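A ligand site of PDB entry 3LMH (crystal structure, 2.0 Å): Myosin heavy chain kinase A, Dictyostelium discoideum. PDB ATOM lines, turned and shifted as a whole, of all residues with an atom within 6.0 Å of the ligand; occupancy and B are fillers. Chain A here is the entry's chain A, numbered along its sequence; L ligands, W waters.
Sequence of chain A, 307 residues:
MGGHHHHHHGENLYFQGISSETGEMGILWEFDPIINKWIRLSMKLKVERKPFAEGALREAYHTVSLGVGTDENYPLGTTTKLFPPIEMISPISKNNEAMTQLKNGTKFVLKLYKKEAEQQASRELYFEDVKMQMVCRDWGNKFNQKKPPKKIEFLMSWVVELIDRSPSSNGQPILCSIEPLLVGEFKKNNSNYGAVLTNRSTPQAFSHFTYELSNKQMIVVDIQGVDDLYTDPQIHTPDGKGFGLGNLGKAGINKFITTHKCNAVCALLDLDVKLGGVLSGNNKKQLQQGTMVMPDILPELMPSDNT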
ATOM      1  N   PHE A  52       2.780  22.204  -5.177  1.00  0.00           N
ATOM      2  CA  PHE A  52       3.022  21.479  -6.427  1.00  0.00           C
ATOM      3  C   PHE A  52       3.297  19.985  -6.208  1.00  0.00           C
ATOM      4  O   PHE A  52       3.342  19.210  -7.163  1.00  0.00           O
ATOM      5  CB  PHE A  52       4.134  22.139  -7.241  1.00  0.00           C
ATOM      6  CG  PHE A  52       5.525  21.944  -6.679  1.00  0.00           C
ATOM      7  CD1 PHE A  52       6.307  20.856  -7.075  1.00  0.00           C
ATOM      8  CD2 PHE A  52       6.062  22.882  -5.794  1.00  0.00           C
ATOM      9  CE1 PHE A  52       7.611  20.686  -6.570  1.00  0.00           C
ATOM     10  CE2 PHE A  52       7.357  22.732  -5.292  1.00  0.00           C
ATOM     11  CZ  PHE A  52       8.134  21.634  -5.669  1.00  0.00           C
ATOM     12  N   ALA A  53       3.495  19.586  -4.958  1.00  0.00           N
ATOM     13  CA  ALA A  53       3.735  18.191  -4.613  1.00  0.00           C
ATOM     14  C   ALA A  53       3.459  17.953  -3.131  1.00  0.00           C
ATOM     15  O   ALA A  53       3.438  18.910  -2.334  1.00  0.00           O
ATOM     16  CB  ALA A  53       5.169  17.782  -4.970  1.00  0.00           C
ATOM     17  N   GLU A  54       3.216  16.704  -2.766  1.00  0.00           N
ATOM     18  CA  GLU A  54       3.146  16.320  -1.357  1.00  0.00           C
ATOM     19  C   GLU A  54       3.846  14.992  -1.069  1.00  0.00           C
ATOM     20  O   GLU A  54       3.908  14.095  -1.925  1.00  0.00           O
ATOM     21  CB  GLU A  54       1.695  16.357  -0.820  1.00  0.00           C
ATOM     22  CG  GLU A  54       0.743  15.265  -1.331  1.00  0.00           C
ATOM     23  CD  GLU A  54      -0.535  15.130  -0.491  1.00  0.00           C
ATOM     24  OE1 GLU A  54      -0.884  16.068   0.278  1.00  0.00           O
ATOM     25  OE2 GLU A  54      -1.219  14.083  -0.605  1.00  0.00           O
ATOM     26  N   GLY A  55       4.405  14.883   0.128  1.00  0.00           N
ATOM     27  CA  GLY A  55       4.976  13.626   0.607  1.00  0.00           C
ATOM     28  C   GLY A  55       4.062  13.134   1.713  1.00  0.00           C
ATOM     29  O   GLY A  55       2.891  13.491   1.753  1.00  0.00           O
ATOM     30  N   ALA A  56       4.600  12.330   2.626  1.00  0.00           N
ATOM     31  CA  ALA A  56       3.835  11.814   3.757  1.00  0.00           C
ATOM     32  C   ALA A  56       3.297  12.915   4.688  1.00  0.00           C
ATOM     33  O   ALA A  56       2.089  12.999   4.914  1.00  0.00           O
ATOM     34  CB  ALA A  56       4.667  10.793   4.538  1.00  0.00           C
ATOM     35  N   LEU A  57       4.183  13.758   5.209  1.00  0.00           N
ATOM     36  CA  LEU A  57       3.802  14.753   6.229  1.00  0.00           C
ATOM     37  C   LEU A  57       3.734  16.194   5.739  1.00  0.00           C
ATOM     38  O   LEU A  57       3.098  17.044   6.377  1.00  0.00           O
ATOM     39  CB  LEU A  57       4.735  14.641   7.436  1.00  0.00           C
ATOM     40  CG  LEU A  57       4.952  13.243   8.025  1.00  0.00           C
ATOM     41  CD1 LEU A  57       5.995  13.260   9.131  1.00  0.00           C
ATOM     42  CD2 LEU A  57       3.620  12.645   8.542  1.00  0.00           C
ATOM     43  N   ARG A  58       4.365  16.475   4.607  1.00  0.00           N
ATOM     44  CA  ARG A  58       4.542  17.848   4.160  1.00  0.00           C
ATOM     45  C   ARG A  58       4.093  18.108   2.726  1.00  0.00           C
ATOM     46  O   ARG A  58       3.982  17.196   1.921  1.00  0.00           O
ATOM     47  CB  ARG A  58       6.014  18.260   4.292  1.00  0.00           C
ATOM     48  CG  ARG A  58       6.548  18.177   5.711  1.00  0.00           C
ATOM     49  CD  ARG A  58       7.997  18.621   5.784  1.00  0.00           C
ATOM     50  NE  ARG A  58       8.889  17.725   5.057  1.00  0.00           N
ATOM     51  CZ  ARG A  58      10.180  17.968   4.839  1.00  0.00           C
ATOM     52  NH1 ARG A  58      10.731  19.084   5.290  1.00  0.00           N
ATOM     53  NH2 ARG A  58      10.928  17.096   4.173  1.00  0.00           N
ATOM     54  N   GLU A  59       3.844  19.382   2.430  1.00  0.00           N
ATOM     55  CA  GLU A  59       3.519  19.827   1.089  1.00  0.00           C
ATOM     56  C   GLU A  59       4.577  20.823   0.627  1.00  0.00           C
ATOM     57  O   GLU A  59       5.055  21.644   1.419  1.00  0.00           O
ATOM     58  CB  GLU A  59       2.117  20.462   1.060  1.00  0.00           C
ATOM     59  CG  GLU A  59       0.992  19.436   1.124  1.00  0.00           C
ATOM     60  CD  GLU A  59      -0.399  20.069   1.193  1.00  0.00           C
ATOM     61  OE1 GLU A  59      -0.603  21.001   2.006  1.00  0.00           O
ATOM     62  OE2 GLU A  59      -1.288  19.600   0.455  1.00  0.00           O
ATOM     63  N   ALA A  60       4.933  20.734  -0.645  1.00  0.00           N
ATOM     64  CA  ALA A  60       5.959  21.593  -1.222  1.00  0.00           C
ATOM     65  C   ALA A  60       5.336  22.679  -2.095  1.00  0.00           C
ATOM     66  O   ALA A  60       4.411  22.411  -2.864  1.00  0.00           O
ATOM     67  CB  ALA A  60       6.940  20.766  -2.026  1.00  0.00           C
ATOM     68  N   VAL A 109      11.949  26.161  -3.129  1.00  0.00           N
ATOM     69  CA  VAL A 109      10.873  25.306  -2.661  1.00  0.00           C
ATOM     70  C   VAL A 109      10.662  25.526  -1.165  1.00  0.00           C
ATOM     71  O   VAL A 109      11.620  25.522  -0.400  1.00  0.00           O
ATOM     72  CB  VAL A 109      11.197  23.820  -2.940  1.00  0.00           C
ATOM     73  CG1 VAL A 109      10.190  22.889  -2.264  1.00  0.00           C
ATOM     74  CG2 VAL A 109      11.277  23.564  -4.456  1.00  0.00           C
ATOM     75  N   LYS A 111       8.521  24.042   2.181  1.00  0.00           N
ATOM     76  CA  LYS A 111       7.818  22.865   2.656  1.00  0.00           C
ATOM     77  C   LYS A 111       7.112  23.154   3.969  1.00  0.00           C
ATOM     78  O   LYS A 111       7.731  23.648   4.907  1.00  0.00           O
ATOM     79  CB  LYS A 111       8.769  21.672   2.793  1.00  0.00           C
ATOM     80  CG  LYS A 111       9.350  21.227   1.461  1.00  0.00           C
ATOM     81  CD  LYS A 111      10.291  20.054   1.595  1.00  0.00           C
ATOM     82  CE  LYS A 111      10.859  19.721   0.218  1.00  0.00           C
ATOM     83  NZ  LYS A 111      11.867  18.628   0.247  1.00  0.00           N
ATOM     84  N   TYR A 113       4.311  21.538   6.923  1.00  0.00           N
ATOM     85  CA  TYR A 113       3.573  20.392   7.450  1.00  0.00           C
ATOM     86  C   TYR A 113       2.080  20.534   7.181  1.00  0.00           C
ATOM     87  O   TYR A 113       1.508  21.598   7.400  1.00  0.00           O
ATOM     88  CB  TYR A 113       3.862  20.196   8.940  1.00  0.00           C
ATOM     89  CG  TYR A 113       5.166  19.460   9.136  1.00  0.00           C
ATOM     90  CD1 TYR A 113       5.202  18.069   9.125  1.00  0.00           C
ATOM     91  CD2 TYR A 113       6.365  20.161   9.270  1.00  0.00           C
ATOM     92  CE1 TYR A 113       6.399  17.378   9.268  1.00  0.00           C
ATOM     93  CE2 TYR A 113       7.572  19.479   9.417  1.00  0.00           C
ATOM     94  CZ  TYR A 113       7.573  18.099   9.416  1.00  0.00           C
ATOM     95  OH  TYR A 113       8.751  17.408   9.553  1.00  0.00           O
ATOM     96  N   LYS A 114       1.469  19.471   6.691  1.00  0.00           N
ATOM     97  CA  LYS A 114       0.073  19.513   6.230  1.00  0.00           C
ATOM     98  C   LYS A 114      -0.922  20.107   7.226  1.00  0.00           C
ATOM     99  O   LYS A 114      -1.574  21.133   6.950  1.00  0.00           O
ATOM    100  CB  LYS A 114      -0.385  18.125   5.785  1.00  0.00           C
ATOM    101  CG  LYS A 114       0.133  17.713   4.424  1.00  0.00           C
ATOM    102  CD  LYS A 114      -0.111  16.244   4.190  1.00  0.00           C
ATOM    103  CE  LYS A 114       0.825  15.702   3.155  1.00  0.00           C
ATOM    104  NZ  LYS A 114       0.630  14.241   2.968  1.00  0.00           N
ATOM    105  N   ASP A 129      15.779  18.881  11.592  1.00  0.00           N
ATOM    106  CA  ASP A 129      15.686  18.348  10.230  1.00  0.00           C
ATOM    107  C   ASP A 129      16.661  19.065   9.291  1.00  0.00           C
ATOM    108  O   ASP A 129      17.325  18.428   8.485  1.00  0.00           O
ATOM    109  CB  ASP A 129      14.243  18.453   9.693  1.00  0.00           C
ATOM    110  CG  ASP A 129      13.916  17.362   8.652  1.00  0.00           C
ATOM    111  OD1 ASP A 129      14.761  16.449   8.413  1.00  0.00           O
ATOM    112  OD2 ASP A 129      12.812  17.417   8.061  1.00  0.00           O
ATOM    113  N   LEU A 155      21.383  19.335  -1.234  1.00  0.00           N
ATOM    114  CA  LEU A 155      21.011  20.728  -1.253  1.00  0.00           C
ATOM    115  C   LEU A 155      21.123  21.299   0.156  1.00  0.00           C
ATOM    116  O   LEU A 155      20.956  20.586   1.156  1.00  0.00           O
ATOM    117  CB  LEU A 155      19.555  20.872  -1.711  1.00  0.00           C
ATOM    118  CG  LEU A 155      19.150  20.389  -3.105  1.00  0.00           C
ATOM    119  CD1 LEU A 155      17.647  20.620  -3.263  1.00  0.00           C
ATOM    120  CD2 LEU A 155      19.943  21.164  -4.163  1.00  0.00           C
ATOM    121  N   GLU A 179      14.361  25.118   0.545  1.00  0.00           N
ATOM    122  CA  GLU A 179      15.537  24.522  -0.082  1.00  0.00           C
ATOM    123  C   GLU A 179      15.506  24.860  -1.574  1.00  0.00           C
ATOM    124  O   GLU A 179      14.442  25.253  -2.087  1.00  0.00           O
ATOM    125  CB  GLU A 179      15.529  23.007   0.134  1.00  0.00           C
ATOM    126  CG  GLU A 179      14.331  22.276  -0.482  1.00  0.00           C
ATOM    127  CD  GLU A 179      14.219  20.849   0.016  1.00  0.00           C
ATOM    128  OE1 GLU A 179      14.160  20.659   1.241  1.00  0.00           O
ATOM    129  OE2 GLU A 179      14.189  19.914  -0.817  1.00  0.00           O
ATOM    130  N   PRO A 180      16.636  24.697  -2.274  1.00  0.00           N
ATOM    131  CA  PRO A 180      16.614  25.063  -3.690  1.00  0.00           C
ATOM    132  C   PRO A 180      15.675  24.166  -4.489  1.00  0.00           C
ATOM    133  O   PRO A 180      15.334  23.059  -4.059  1.00  0.00           O
ATOM    134  CB  PRO A 180      18.081  24.844  -4.130  1.00  0.00           C
ATOM    135  CG  PRO A 180      18.859  24.887  -2.844  1.00  0.00           C
ATOM    136  CD  PRO A 180      17.959  24.207  -1.871  1.00  0.00           C
ATOM    137  N   LEU A 181      15.267  24.660  -5.657  1.00  0.00           N
ATOM    138  CA  LEU A 181      14.400  23.903  -6.537  1.00  0.00           C
ATOM    139  C   LEU A 181      15.213  22.871  -7.331  1.00  0.00           C
ATOM    140  O   LEU A 181      16.225  23.220  -7.927  1.00  0.00           O
ATOM    141  CB  LEU A 181      13.684  24.844  -7.502  1.00  0.00           C
ATOM    142  CG  LEU A 181      12.800  24.191  -8.586  1.00  0.00           C
ATOM    143  CD1 LEU A 181      11.582  23.478  -8.014  1.00  0.00           C
ATOM    144  CD2 LEU A 181      12.378  25.253  -9.606  1.00  0.00           C
ATOM    145  N   LEU A 182      14.776  21.613  -7.287  1.00  0.00           N
ATOM    146  CA  LEU A 182      15.385  20.588  -8.134  1.00  0.00           C
ATOM    147  C   LEU A 182      14.651  20.575  -9.458  1.00  0.00           C
ATOM    148  O   LEU A 182      13.424  20.535  -9.491  1.00  0.00           O
ATOM    149  CB  LEU A 182      15.310  19.218  -7.477  1.00  0.00           C
ATOM    150  CG  LEU A 182      16.172  18.998  -6.220  1.00  0.00           C
ATOM    151  CD1 LEU A 182      15.714  17.749  -5.492  1.00  0.00           C
ATOM    152  CD2 LEU A 182      17.640  18.938  -6.575  1.00  0.00           C
ATOM    153  N   VAL A 183      15.398  20.602 -10.557  1.00  0.00           N
ATOM    154  CA  VAL A 183      14.801  20.534 -11.892  1.00  0.00           C
ATOM    155  C   VAL A 183      15.073  19.155 -12.468  1.00  0.00           C
ATOM    156  O   VAL A 183      16.229  18.751 -12.598  1.00  0.00           O
ATOM    157  CB  VAL A 183      15.371  21.653 -12.796  1.00  0.00           C
ATOM    158  CG1 VAL A 183      14.960  21.443 -14.274  1.00  0.00           C
ATOM    159  CG2 VAL A 183      14.935  23.019 -12.301  1.00  0.00           C
ATOM    160  N   PHE A 186      12.189  13.708 -10.011  1.00  0.00           N
ATOM    161  CA  PHE A 186      12.508  13.423  -8.628  1.00  0.00           C
ATOM    162  C   PHE A 186      12.300  11.934  -8.338  1.00  0.00           C
ATOM    163  O   PHE A 186      11.210  11.411  -8.531  1.00  0.00           O
ATOM    164  CB  PHE A 186      11.616  14.266  -7.703  1.00  0.00           C
ATOM    165  CG  PHE A 186      12.052  14.286  -6.260  1.00  0.00           C
ATOM    166  CD1 PHE A 186      12.720  15.406  -5.742  1.00  0.00           C
ATOM    167  CD2 PHE A 186      11.792  13.208  -5.408  1.00  0.00           C
ATOM    168  CE1 PHE A 186      13.107  15.440  -4.409  1.00  0.00           C
ATOM    169  CE2 PHE A 186      12.179  13.242  -4.075  1.00  0.00           C
ATOM    170  CZ  PHE A 186      12.840  14.353  -3.569  1.00  0.00           C
ATOM    171  N   LYS A 188      13.069   8.695  -5.408  1.00  0.00           N
ATOM    172  CA  LYS A 188      13.482   8.168  -4.124  1.00  0.00           C
ATOM    173  C   LYS A 188      14.224   6.848  -4.346  1.00  0.00           C
ATOM    174  O   LYS A 188      13.709   5.945  -4.993  1.00  0.00           O
ATOM    175  CB  LYS A 188      12.250   7.971  -3.238  1.00  0.00           C
ATOM    176  CG  LYS A 188      12.525   7.586  -1.797  1.00  0.00           C
ATOM    177  CD  LYS A 188      11.285   7.861  -0.962  1.00  0.00           C
ATOM    178  CE  LYS A 188      11.507   7.518   0.485  1.00  0.00           C
ATOM    179  NZ  LYS A 188      10.522   8.233   1.359  1.00  0.00           N
ATOM    180  N   GLN A 224      17.204  10.573  -1.912  1.00  0.00           N
ATOM    181  CA  GLN A 224      16.190  10.943  -2.891  1.00  0.00           C
ATOM    182  C   GLN A 224      16.495  12.324  -3.445  1.00  0.00           C
ATOM    183  O   GLN A 224      17.076  13.184  -2.746  1.00  0.00           O
ATOM    184  CB  GLN A 224      14.806  10.945  -2.239  1.00  0.00           C
ATOM    185  CG  GLN A 224      14.674  11.888  -1.048  1.00  0.00           C
ATOM    186  CD  GLN A 224      13.345  11.767  -0.348  1.00  0.00           C
ATOM    187  OE1 GLN A 224      12.338  11.400  -0.965  1.00  0.00           O
ATOM    188  NE2 GLN A 224      13.319  12.095   0.933  1.00  0.00           N
ATOM    189  N   THR A 231      18.021  15.543  -1.484  1.00  0.00           N
ATOM    190  CA  THR A 231      17.358  16.356  -0.488  1.00  0.00           C
ATOM    191  C   THR A 231      16.547  15.494   0.479  1.00  0.00           C
ATOM    192  O   THR A 231      16.311  14.305   0.219  1.00  0.00           O
ATOM    193  CB  THR A 231      16.504  17.476  -1.150  1.00  0.00           C
ATOM    194  OG1 THR A 231      16.188  18.479  -0.172  1.00  0.00           O
ATOM    195  CG2 THR A 231      15.218  16.897  -1.770  1.00  0.00           C
ATOM    196  N   PHD A 232      16.149  16.077   1.607  1.00  0.00           N
ATOM    197  CA  PHD A 232      15.372  15.353   2.617  1.00  0.00           C
ATOM    198  C   PHD A 232      15.886  13.960   2.921  1.00  0.00           C
ATOM    199  O   PHD A 232      15.132  12.985   2.838  1.00  0.00           O
ATOM    200  CB  PHD A 232      13.892  15.376   2.225  1.00  0.00           C
ATOM    201  CG  PHD A 232      12.972  14.726   3.265  1.00  0.00           C
ATOM    202  OD1 PHD A 232      13.048  15.058   4.693  1.00  0.00           O
ATOM    203  OD2 PHD A 232      12.140  13.930   2.845  1.00  0.00           O
ATOM    204  P   PHD A 232      12.630  14.167   6.012  1.00  0.00           P
ATOM    205  OP1 PHD A 232      11.899  12.970   5.453  1.00  0.00           O
ATOM    206  OP2 PHD A 232      13.978  13.922   6.707  1.00  0.00           O
ATOM    207  OP3 PHD A 232      11.723  15.071   6.859  1.00  0.00           O
HETATM  208  P1  LIG L   1       7.811  14.624   3.559  1.00  0.00           P
HETATM  209  O1  LIG L   1       6.344  14.329   3.597  1.00  0.00           O
HETATM  210  O2  LIG L   1       8.246  15.348   4.819  1.00  0.00           O
HETATM  211  O3  LIG L   1       8.690  13.451   3.213  1.00  0.00           O
HETATM  212  P2  LIG L   1       9.053  15.470   1.050  1.00  0.00           P
HETATM  213  O4  LIG L   1      10.406  16.072   1.388  1.00  0.00           O
HETATM  214  O5  LIG L   1       8.999  13.998   0.676  1.00  0.00           O
HETATM  215  O6  LIG L   1       8.033  15.690   2.318  1.00  0.00           O
HETATM  216  O7  LIG L   1       8.532  16.360  -0.212  1.00  0.00           O
HETATM  217  C1  LIG L   1       7.407  16.020  -1.021  1.00  0.00           C
HETATM  218  C2  LIG L   1       7.671  15.968  -2.531  1.00  0.00           C
HETATM  219  O8  LIG L   1       8.073  17.227  -3.108  1.00  0.00           O
HETATM  220  C3  LIG L   1       8.750  14.991  -2.960  1.00  0.00           C
HETATM  221  O9  LIG L   1       8.216  13.680  -3.083  1.00  0.00           O
HETATM  222  C4  LIG L   1       9.165  15.523  -4.314  1.00  0.00           C
HETATM  223  O10 LIG L   1       8.198  15.070  -5.274  1.00  0.00           O
HETATM  224  C5  LIG L   1       9.003  17.027  -4.184  1.00  0.00           C
HETATM  225  N1  LIG L   1      10.247  17.782  -3.847  1.00  0.00           N
HETATM  226  C6  LIG L   1      10.869  17.751  -2.641  1.00  0.00           C
HETATM  227  N2  LIG L   1      11.949  18.567  -2.616  1.00  0.00           N
HETATM  228  C7  LIG L   1      12.028  19.166  -3.821  1.00  0.00           C
HETATM  229  C8  LIG L   1      12.929  20.140  -4.457  1.00  0.00           C
HETATM  230  N3  LIG L   1      13.987  20.655  -3.782  1.00  0.00           N
HETATM  231  N4  LIG L   1      12.663  20.491  -5.728  1.00  0.00           N
HETATM  232  C9  LIG L   1      11.619  19.976  -6.410  1.00  0.00           C
HETATM  233  N5  LIG L   1      10.768  19.083  -5.894  1.00  0.00           N
HETATM  234  C10 LIG L   1      10.904  18.636  -4.622  1.00  0.00           C
HETATM  235  O   HOH W   1       8.865  15.177   7.655  1.00  0.00           O
HETATM  236  O   HOH W   2       9.798  11.713  -0.530  1.00  0.00           O
HETATM  237  O   HOH W   3      10.662  11.055   2.231  1.00  0.00           O
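The backbone NH (N) of Arg 58 sits at hydrogen-bond distance from an oxygen (O1) of the ligand (3.1 Å).
The backbone carbonyl oxygen (O) of Pro 180 sits at hydrogen-bond distance from a nitrogen (N3) of the ligand (2.8 Å).
N4 of the ligand is in hydrogen-bond range of N of Leu 182, 2.9 Å away.
The backbone NH of Leu 57 is in hydrogen-bond range of an oxygen (O1) of the ligand (2.8 Å).
OE2 of Glu 179 lies within hydrogen-bond range of N3 of the ligand.
N of Ala 56 sits at hydrogen-bond distance from O1 of the ligand (2.8 Å).
An oxygen (O2) of the ligand lies within salt-bridge range of the guanidinium group (NE) of Arg 58 (2.5 Å).
An oxygen (O4) of the ligand lies within salt-bridge range of the side-chain amino group (NZ) of Lys 111.
OD2 of Asp 129 sits close to OP3 of PHD 232 (2.9 Å).
The side-chain carboxylate (OE1) of Glu 54 is in salt-bridge range of the side-chain amino group (NZ) of Lys 114.
O of Ala 53 lies within hydrogen-bond range of N of Ala 60, at 2.9 Å.
The side-chain amino group of Lys 111 lies within salt-bridge range of the side-chain carboxylate of Glu 179.
The backbone carbonyl oxygen of Leu 57 lies within hydrogen-bond range of the backbone NH of Lys 114 (2.9 Å).
O of PHD 232 lies within hydrogen-bond range of NE2 of Gln 224, 2.8 Å away.
OD2 of Asp 129 lies within salt-bridge range of NH1 of Arg 58, at 3.8 Å.
The side-chain carboxylate (OE2) of Glu 179 sits at hydrogen-bond distance from the side-chain hydroxyl (OG1) of Thr 231 (2.5 Å).
An oxygen (O4) of the ligand lies close to OD2 of PHD 232, 3.1 Å away.
Residues that only touch the ligand: Phe 52 (3.6 Å), Ala 53 (3.5 Å), Glu 54 (3.7 Å), Gly 55 (3.2 Å), Ala 60 (3.9 Å), Val 109 (3.6 Å), Leu 155 (3.7 Å), Leu 181 (3.8 Å), Phe 186 (3.7 Å) and Thr 231 (3.8 Å).
Hydrophobic or aromatic side chains within 4 Å of the ligand: Phe 52, Ala 53, Ala 60, Val 109, Leu 155, Leu 181, Leu 182 and Phe 186.
Of the 25 residues printed, 18 come within 4 Å of the ligand.
Water W2 bridges OE1 of Gln 224 (2.6 Å) and O5 of the ligand (2.7 Å).
Water W1 lies within hydrogen-bond range of an oxygen (O2) of the ligand (2.9 Å), the side-chain hydroxyl of Tyr 113 (2.9 Å) and OP3 of PHD 232 (3.0 Å).
Water W3 lies within hydrogen-bond range of the side-chain amino group of Lys 188 (3.0 Å), the side-chain amide nitrogen of Gln 224 (3.1 Å), an oxygen (O3) of the ligand (3.3 Å) and OD2 of PHD 232 (3.3 Å).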
